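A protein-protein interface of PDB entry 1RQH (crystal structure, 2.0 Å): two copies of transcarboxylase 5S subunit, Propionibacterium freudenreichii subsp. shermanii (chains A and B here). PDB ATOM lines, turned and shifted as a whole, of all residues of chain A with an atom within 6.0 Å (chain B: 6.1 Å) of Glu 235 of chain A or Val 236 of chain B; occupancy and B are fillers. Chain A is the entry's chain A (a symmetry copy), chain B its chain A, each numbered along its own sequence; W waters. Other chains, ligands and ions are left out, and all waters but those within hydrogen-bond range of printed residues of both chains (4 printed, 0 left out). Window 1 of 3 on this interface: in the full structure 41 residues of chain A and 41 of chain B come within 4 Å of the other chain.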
ATOM      1  N   GLY A 232       3.125  18.107 -13.455  1.00  0.00           N
ATOM      2  CA  GLY A 232       4.480  18.582 -13.236  1.00  0.00           C
ATOM      3  C   GLY A 232       5.552  18.235 -14.258  1.00  0.00           C
ATOM      4  O   GLY A 232       6.724  18.488 -13.999  1.00  0.00           O
ATOM      5  N   VAL A 233       5.179  17.708 -15.427  1.00  0.00           N
ATOM      6  CA  VAL A 233       6.187  17.314 -16.422  1.00  0.00           C
ATOM      7  C   VAL A 233       6.116  18.186 -17.688  1.00  0.00           C
ATOM      8  O   VAL A 233       6.994  18.074 -18.552  1.00  0.00           O
ATOM      9  CB  VAL A 233       5.963  15.850 -16.942  1.00  0.00           C
ATOM     10  CG1 VAL A 233       5.671  14.883 -15.795  1.00  0.00           C
ATOM     11  CG2 VAL A 233       4.797  15.822 -17.934  1.00  0.00           C
ATOM     12  N   THR A 234       5.127  19.064 -17.796  1.00  0.00           N
ATOM     13  CA  THR A 234       4.920  19.771 -19.065  1.00  0.00           C
ATOM     14  C   THR A 234       5.861  20.931 -19.355  1.00  0.00           C
ATOM     15  O   THR A 234       5.932  21.329 -20.520  1.00  0.00           O
ATOM     16  CB  THR A 234       3.460  20.219 -19.232  1.00  0.00           C
ATOM     17  OG1 THR A 234       3.097  21.111 -18.173  1.00  0.00           O
ATOM     18  CG2 THR A 234       2.548  18.989 -19.231  1.00  0.00           C
ATOM     19  N   GLU A 235       6.570  21.510 -18.393  1.00  0.00           N
ATOM     20  CA  GLU A 235       7.468  22.583 -18.823  1.00  0.00           C
ATOM     21  C   GLU A 235       8.615  21.943 -19.615  1.00  0.00           C
ATOM     22  O   GLU A 235       9.203  22.561 -20.509  1.00  0.00           O
ATOM     23  CB  GLU A 235       8.003  23.370 -17.625  1.00  0.00           C
ATOM     24  CG  GLU A 235       8.691  24.498 -18.063  1.00  0.00           C
ATOM     25  CD  GLU A 235       9.021  25.465 -16.931  1.00  0.00           C
ATOM     26  OE1 GLU A 235       8.088  26.010 -16.313  1.00  0.00           O
ATOM     27  OE2 GLU A 235      10.216  25.677 -16.651  1.00  0.00           O
ATOM     28  N   VAL A 236       8.935  20.693 -19.285  1.00  0.00           N
ATOM     29  CA  VAL A 236       9.977  19.987 -20.021  1.00  0.00           C
ATOM     30  C   VAL A 236       9.413  19.674 -21.407  1.00  0.00           C
ATOM     31  O   VAL A 236      10.119  19.695 -22.409  1.00  0.00           O
ATOM     32  CB  VAL A 236      10.384  18.665 -19.313  1.00  0.00           C
ATOM     33  CG1 VAL A 236      11.438  17.936 -20.132  1.00  0.00           C
ATOM     34  CG2 VAL A 236      10.935  18.962 -17.926  1.00  0.00           C
ATOM     35  N   SER A 237       8.111  19.413 -21.454  1.00  0.00           N
ATOM     36  CA  SER A 237       7.442  19.123 -22.717  1.00  0.00           C
ATOM     37  C   SER A 237       7.493  20.371 -23.595  1.00  0.00           C
ATOM     38  O   SER A 237       7.703  20.279 -24.806  1.00  0.00           O
ATOM     39  CB  SER A 237       5.992  18.706 -22.448  1.00  0.00           C
ATOM     40  OG  SER A 237       5.952  17.523 -21.659  1.00  0.00           O
ATOM     41  N   LEU A 238       7.308  21.536 -22.976  1.00  0.00           N
ATOM     42  CA  LEU A 238       7.361  22.804 -23.695  1.00  0.00           C
ATOM     43  C   LEU A 238       8.743  22.981 -24.341  1.00  0.00           C
ATOM     44  O   LEU A 238       8.831  23.403 -25.493  1.00  0.00           O
ATOM     45  CB  LEU A 238       7.082  23.955 -22.731  1.00  0.00           C
ATOM     46  CG  LEU A 238       5.694  24.590 -22.801  1.00  0.00           C
ATOM     47  CD1 LEU A 238       4.640  23.530 -22.629  1.00  0.00           C
ATOM     48  CD2 LEU A 238       5.563  25.674 -21.732  1.00  0.00           C
ATOM     49  N   MET A 239       9.814  22.667 -23.613  1.00  0.00           N
ATOM     50  CA  MET A 239      11.173  22.796 -24.159  1.00  0.00           C
ATOM     51  C   MET A 239      11.321  21.851 -25.359  1.00  0.00           C
ATOM     52  O   MET A 239      11.853  22.235 -26.396  1.00  0.00           O
ATOM     53  CB  MET A 239      12.213  22.448 -23.069  1.00  0.00           C
ATOM     54  CG  MET A 239      13.518  22.607 -23.530  1.00  0.00           C
ATOM     55  SD  MET A 239      14.077  24.353 -23.703  1.00  0.00           S
ATOM     56  CE  MET A 239      14.221  24.481 -25.469  1.00  0.00           C
ATOM     57  N   LYS A 240      10.836  20.619 -25.222  1.00  0.00           N
ATOM     58  CA  LYS A 240      10.908  19.645 -26.313  1.00  0.00           C
ATOM     59  C   LYS A 240      10.067  20.104 -27.492  1.00  0.00           C
ATOM     60  O   LYS A 240      10.452  19.892 -28.644  1.00  0.00           O
ATOM     61  CB  LYS A 240      10.428  18.268 -25.826  1.00  0.00           C
ATOM     62  CG  LYS A 240      11.350  17.715 -24.943  1.00  0.00           C
ATOM     63  CD  LYS A 240      12.559  17.516 -25.599  1.00  0.00           C
ATOM     64  CE  LYS A 240      13.566  17.070 -24.751  1.00  0.00           C
ATOM     65  NZ  LYS A 240      14.843  16.991 -25.514  1.00  0.00           N
ATOM     66  N   LEU A 258       1.232  27.061 -11.931  1.00  0.00           N
ATOM     67  CA  LEU A 258       1.504  25.735 -11.368  1.00  0.00           C
ATOM     68  C   LEU A 258       0.228  25.057 -10.878  1.00  0.00           C
ATOM     69  O   LEU A 258      -0.879  25.580 -11.037  1.00  0.00           O
ATOM     70  CB  LEU A 258       2.558  25.844 -10.255  1.00  0.00           C
ATOM     71  CG  LEU A 258       3.896  26.402 -10.769  1.00  0.00           C
ATOM     72  CD1 LEU A 258       4.975  26.270  -9.693  1.00  0.00           C
ATOM     73  CD2 LEU A 258       4.310  25.651 -12.027  1.00  0.00           C
ATOM     74  N   ASN A 263       2.293  26.333 -16.707  1.00  0.00           N
ATOM     75  CA  ASN A 263       3.700  26.633 -16.437  1.00  0.00           C
ATOM     76  C   ASN A 263       3.856  28.153 -16.424  1.00  0.00           C
ATOM     77  O   ASN A 263       3.151  28.858 -17.150  1.00  0.00           O
ATOM     78  CB  ASN A 263       4.574  25.963 -17.498  1.00  0.00           C
ATOM     79  CG  ASN A 263       4.432  24.450 -17.479  1.00  0.00           C
ATOM     80  OD1 ASN A 263       4.772  23.797 -16.492  1.00  0.00           O
ATOM     81  ND2 ASN A 263       3.908  23.886 -18.560  1.00  0.00           N
ATOM     82  N   PRO A 264       4.784  28.675 -15.606  1.00  0.00           N
ATOM     83  CA  PRO A 264       4.999  30.121 -15.487  1.00  0.00           C
ATOM     84  C   PRO A 264       5.587  30.852 -16.679  1.00  0.00           C
ATOM     85  O   PRO A 264       6.611  30.458 -17.235  1.00  0.00           O
ATOM     86  CB  PRO A 264       5.884  30.243 -14.240  1.00  0.00           C
ATOM     87  CG  PRO A 264       5.887  28.852 -13.625  1.00  0.00           C
ATOM     88  CD  PRO A 264       5.791  27.958 -14.812  1.00  0.00           C
ATOM     89  N   SER A 267       9.206  31.907 -16.129  1.00  0.00           N
ATOM     90  CA  SER A 267      10.082  30.732 -16.086  1.00  0.00           C
ATOM     91  C   SER A 267      10.344  30.221 -17.506  1.00  0.00           C
ATOM     92  O   SER A 267      11.483  29.931 -17.874  1.00  0.00           O
ATOM     93  CB  SER A 267       9.426  29.632 -15.241  1.00  0.00           C
ATOM     94  OG  SER A 267       9.233  30.060 -13.898  1.00  0.00           O
ATOM     95  N   VAL A 268       9.294  30.118 -18.312  1.00  0.00           N
ATOM     96  CA  VAL A 268       9.456  29.637 -19.681  1.00  0.00           C
ATOM     97  C   VAL A 268      10.323  30.609 -20.481  1.00  0.00           C
ATOM     98  O   VAL A 268      11.130  30.187 -21.311  1.00  0.00           O
ATOM     99  CB  VAL A 268       8.088  29.456 -20.362  1.00  0.00           C
ATOM    100  CG1 VAL A 268       8.257  29.327 -21.868  1.00  0.00           C
ATOM    101  CG2 VAL A 268       7.401  28.217 -19.787  1.00  0.00           C
ATOM    102  N   MET A 271      14.065  30.248 -19.118  1.00  0.00           N
ATOM    103  CA  MET A 271      14.737  28.967 -19.368  1.00  0.00           C
ATOM    104  C   MET A 271      15.388  28.886 -20.753  1.00  0.00           C
ATOM    105  O   MET A 271      16.202  27.993 -20.970  1.00  0.00           O
ATOM    106  CB  MET A 271      13.744  27.806 -19.230  1.00  0.00           C
ATOM    107  CG  MET A 271      12.826  27.770 -20.272  1.00  0.00           C
ATOM    108  SD  MET A 271      11.656  26.372 -20.056  1.00  0.00           S
ATOM    109  CE  MET A 271      10.958  26.148 -21.689  1.00  0.00           C
ATOM    110  N   PRO B 203      18.795  25.678 -18.240  1.00  0.00           N
ATOM    111  CA  PRO B 203      19.016  24.512 -19.100  1.00  0.00           C
ATOM    112  C   PRO B 203      20.330  24.408 -19.868  1.00  0.00           C
ATOM    113  O   PRO B 203      21.016  23.390 -19.776  1.00  0.00           O
ATOM    114  CB  PRO B 203      17.811  24.552 -20.036  1.00  0.00           C
ATOM    115  CG  PRO B 203      16.734  25.081 -19.140  1.00  0.00           C
ATOM    116  CD  PRO B 203      17.438  26.221 -18.435  1.00  0.00           C
ATOM    117  N   GLY B 232      11.541  28.088 -10.962  1.00  0.00           N
ATOM    118  CA  GLY B 232      10.688  27.367 -11.890  1.00  0.00           C
ATOM    119  C   GLY B 232      11.274  26.903 -13.215  1.00  0.00           C
ATOM    120  O   GLY B 232      10.521  26.445 -14.069  1.00  0.00           O
ATOM    121  N   VAL B 233      12.595  26.966 -13.391  1.00  0.00           N
ATOM    122  CA  VAL B 233      13.197  26.571 -14.673  1.00  0.00           C
ATOM    123  C   VAL B 233      14.065  25.310 -14.538  1.00  0.00           C
ATOM    124  O   VAL B 233      14.516  24.771 -15.556  1.00  0.00           O
ATOM    125  CB  VAL B 233      14.178  27.666 -15.226  1.00  0.00           C
ATOM    126  CG1 VAL B 233      13.580  29.068 -15.114  1.00  0.00           C
ATOM    127  CG2 VAL B 233      15.499  27.617 -14.454  1.00  0.00           C
ATOM    128  N   THR B 234      14.274  24.813 -13.324  1.00  0.00           N
ATOM    129  CA  THR B 234      15.248  23.731 -13.140  1.00  0.00           C
ATOM    130  C   THR B 234      14.790  22.334 -13.534  1.00  0.00           C
ATOM    131  O   THR B 234      15.659  21.475 -13.701  1.00  0.00           O
ATOM    132  CB  THR B 234      15.818  23.719 -11.715  1.00  0.00           C
ATOM    133  OG1 THR B 234      14.764  23.521 -10.767  1.00  0.00           O
ATOM    134  CG2 THR B 234      16.538  25.043 -11.444  1.00  0.00           C
ATOM    135  N   GLU B 235      13.503  22.039 -13.680  1.00  0.00           N
ATOM    136  CA  GLU B 235      13.210  20.670 -14.106  1.00  0.00           C
ATOM    137  C   GLU B 235      13.654  20.531 -15.567  1.00  0.00           C
ATOM    138  O   GLU B 235      14.023  19.444 -16.028  1.00  0.00           O
ATOM    139  CB  GLU B 235      11.722  20.349 -13.953  1.00  0.00           C
ATOM    140  CG  GLU B 235      11.499  18.993 -14.176  1.00  0.00           C
ATOM    141  CD  GLU B 235      10.093  18.553 -13.784  1.00  0.00           C
ATOM    142  OE1 GLU B 235       9.748  18.633 -12.590  1.00  0.00           O
ATOM    143  OE2 GLU B 235       9.326  18.132 -14.670  1.00  0.00           O
ATOM    144  N   VAL B 236      13.620  21.640 -16.303  1.00  0.00           N
ATOM    145  CA  VAL B 236      14.077  21.613 -17.688  1.00  0.00           C
ATOM    146  C   VAL B 236      15.598  21.457 -17.656  1.00  0.00           C
ATOM    147  O   VAL B 236      16.195  20.797 -18.499  1.00  0.00           O
ATOM    148  CB  VAL B 236      13.702  22.919 -18.440  1.00  0.00           C
ATOM    149  CG1 VAL B 236      14.232  22.872 -19.865  1.00  0.00           C
ATOM    150  CG2 VAL B 236      12.190  23.093 -18.468  1.00  0.00           C
ATOM    151  N   SER B 237      16.216  22.053 -16.643  1.00  0.00           N
ATOM    152  CA  SER B 237      17.662  21.962 -16.480  1.00  0.00           C
ATOM    153  C   SER B 237      18.033  20.508 -16.198  1.00  0.00           C
ATOM    154  O   SER B 237      19.037  20.005 -16.707  1.00  0.00           O
ATOM    155  CB  SER B 237      18.110  22.870 -15.329  1.00  0.00           C
ATOM    156  OG  SER B 237      17.794  24.226 -15.614  1.00  0.00           O
ATOM    157  N   LEU B 238      17.212  19.836 -15.393  1.00  0.00           N
ATOM    158  CA  LEU B 238      17.436  18.431 -15.067  1.00  0.00           C
ATOM    159  C   LEU B 238      17.417  17.586 -16.349  1.00  0.00           C
ATOM    160  O   LEU B 238      18.262  16.708 -16.518  1.00  0.00           O
ATOM    161  CB  LEU B 238      16.355  17.947 -14.104  1.00  0.00           C
ATOM    162  CG  LEU B 238      16.757  17.794 -12.638  1.00  0.00           C
ATOM    163  CD1 LEU B 238      17.331  19.089 -12.130  1.00  0.00           C
ATOM    164  CD2 LEU B 238      15.547  17.366 -11.808  1.00  0.00           C
ATOM    165  N   MET B 239      16.465  17.842 -17.247  1.00  0.00           N
ATOM    166  CA  MET B 239      16.382  17.089 -18.508  1.00  0.00           C
ATOM    167  C   MET B 239      17.658  17.336 -19.323  1.00  0.00           C
ATOM    168  O   MET B 239      18.243  16.406 -19.868  1.00  0.00           O
ATOM    169  CB  MET B 239      15.137  17.537 -19.306  1.00  0.00           C
ATOM    170  CG  MET B 239      14.990  16.812 -20.486  1.00  0.00           C
ATOM    171  SD  MET B 239      14.400  15.081 -20.269  1.00  0.00           S
ATOM    172  CE  MET B 239      15.848  14.173 -20.755  1.00  0.00           C
ATOM    173  N   LYS B 240      18.097  18.592 -19.393  1.00  0.00           N
ATOM    174  CA  LYS B 240      19.315  18.933 -20.129  1.00  0.00           C
ATOM    175  C   LYS B 240      20.528  18.292 -19.477  1.00  0.00           C
ATOM    176  O   LYS B 240      21.449  17.865 -20.176  1.00  0.00           O
ATOM    177  CB  LYS B 240      19.488  20.461 -20.185  1.00  0.00           C
ATOM    178  CG  LYS B 240      18.531  21.030 -21.017  1.00  0.00           C
ATOM    179  CD  LYS B 240      18.701  20.555 -22.312  1.00  0.00           C
ATOM    180  CE  LYS B 240      17.709  20.993 -23.182  1.00  0.00           C
ATOM    181  NZ  LYS B 240      17.908  20.350 -24.510  1.00  0.00           N
ATOM    182  N   ALA B 241      20.547  18.245 -18.146  1.00  0.00           N
ATOM    183  CA  ALA B 241      21.675  17.627 -17.453  1.00  0.00           C
ATOM    184  C   ALA B 241      21.695  16.136 -17.783  1.00  0.00           C
ATOM    185  O   ALA B 241      22.760  15.542 -17.934  1.00  0.00           O
ATOM    186  CB  ALA B 241      21.561  17.833 -15.934  1.00  0.00           C
ATOM    187  N   ASN B 263      12.217  19.939  -7.488  1.00  0.00           N
ATOM    188  CA  ASN B 263      11.351  19.374  -8.523  1.00  0.00           C
ATOM    189  C   ASN B 263      10.821  18.038  -8.007  1.00  0.00           C
ATOM    190  O   ASN B 263      11.513  17.339  -7.262  1.00  0.00           O
ATOM    191  CB  ASN B 263      12.143  19.229  -9.823  1.00  0.00           C
ATOM    192  CG  ASN B 263      12.638  20.569 -10.342  1.00  0.00           C
ATOM    193  OD1 ASN B 263      11.843  21.445 -10.685  1.00  0.00           O
ATOM    194  ND2 ASN B 263      13.953  20.745 -10.380  1.00  0.00           N
HETATM  195  O   HOH W   1      11.160  23.553 -14.467  1.00  0.00           O
HETATM  196  O   HOH W   2       7.700  20.589 -15.886  1.00  0.00           O
HETATM  197  O   HOH W   3       7.918  25.815 -12.983  1.00  0.00           O
HETATM  198  O   HOH W   4       6.965  20.274 -11.740  1.00  0.00           O
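Glu 235 of chain A touches just these residues of chain B: Gly 232, Val 233 and Val 236. Of the printed residues of chain A, Gly 232 of chain B touches Glu 235 and Ser 267. Printed residues of chain B within 4 Å of Val 233 of chain A: Glu 235. Of the printed residues of chain B, Ser 267 of chain A touches Gly 232 (3.6 Å) and Val 233 (3.6 Å). Printed residues of chain A within 4 Å of Val 233 of chain B: Glu 235 (3.7 Å) and Ser 267 (3.6 Å). Val 268 of chain A touches none of the printed residues of chain B.
Among the printed residues, pairs that only touch across the chains: Met 271 of chain A with Pro 203 of chain B (3.3 Å), Ser 267 of chain A with Gly 232 of chain B (3.6 Å), Ser 267 of chain A with Val 233 of chain B (3.6 Å), Val 236 of chain A with Glu 235 of chain B (3.7 Å), Glu 235 of chain A with Val 236 of chain B (3.7 Å), Met 271 of chain A with Val 236 of chain B (3.7 Å), Val 233 of chain A with Glu 235 of chain B (3.7 Å), Glu 235 of chain A with Val 233 of chain B (3.7 Å), Val 236 of chain A with Met 239 of chain B (3.7 Å) and Met 239 of chain A with Val 236 of chain B (3.7 Å).
Water W4 bridges O of Gly 232 of chain A (2.9 Å) and OE1 of Glu 235 of chain B (3.3 Å). Water W3 lies within hydrogen-bond range of the backbone carbonyl oxygen of Gly 232 of chain B (2.9 Å) and the side-chain carboxylate of Glu 235 of chain A (3.3 Å). Water W1 lies within hydrogen-bond range of the backbone NH of Glu 235 of chain B (2.9 Å), the backbone carbonyl oxygen of Gly 232 of chain B (3.0 Å) and the side-chain carboxylate of Glu 235 of chain A (3.2 Å). Water W2 lies within hydrogen-bond range of N of Glu 235 of chain A (2.9 Å), O of Gly 232 of chain A (3.0 Å) and OE2 of Glu 235 of chain B (3.2 Å).
Gly 232 of chain A touches Glu 235 of chain B, and with the chains exchanged Glu 235 of chain A touches Gly 232 of chain B. Val 233 of chain A touches Glu 235 of chain B, and with the chains exchanged Glu 235 of chain A touches Val 233 of chain B. Glu 235 of chain A touches Val 236 of chain B, and with the chains exchanged Val 236 of chain A touches Glu 235 of chain B. Val 236 of chain A touches Met 239 of chain B, and with the chains exchanged Met 239 of chain A touches Val 236 of chain B. Positions printed for both chains: 232, 233, 234, 235, 236, 237, 238, 239, 240 and 263. Of the 12 pairs that touch across the chains among the printed residues, 8 have their exchanged pair printed and touching as well.
The backbone carbonyl oxygen (O) of Val 233 of chain B lies within hydrogen-bond range of the side-chain hydroxyl (OG) of Ser 237 of chain B, at 3.3 Å. OD1 of Asn 263 of chain B lies close to N of Glu 235 of chain B. OG of Ser 237 of chain A sits at hydrogen-bond distance from O of Val 233 of chain A, at 3.3 Å. The backbone NH of Glu 235 of chain A lies close to the side-chain amide oxygen of Asn 263 of chain A.
The backbone carbonyl oxygen (O) of Gly 232 of chain B sits close to the side-chain carboxylate (OE2) of Glu 235 of chain A, 2.7 Å away. The side-chain carboxylate (OE2) of Glu 235 of chain B lies close to the backbone carbonyl oxygen (O) of Gly 232 of chain A, 2.7 Å away.
Printed residues of chain B that touch a printed residue of chain A: Pro 203, Gly 232, Val 233, Glu 235, Val 236 and Met 239. Hydrophobic or aromatic side chains of chain B that line the printed part of chain A: Pro 203, Val 233, Val 236 and Met 239. Of the 15 printed residues of chain A, 7 touch a printed residue of chain B. Hydrophobic or aromatic side chains of chain A that line the printed part of chain B: Val 236, Met 239 and Met 271. Among the printed residues, 12 pairs touch across the chains. Among the printed residues, no Asp or Glu carboxylate lies within 4 Å of a Lys or Arg side-chain nitrogen of the other chain.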
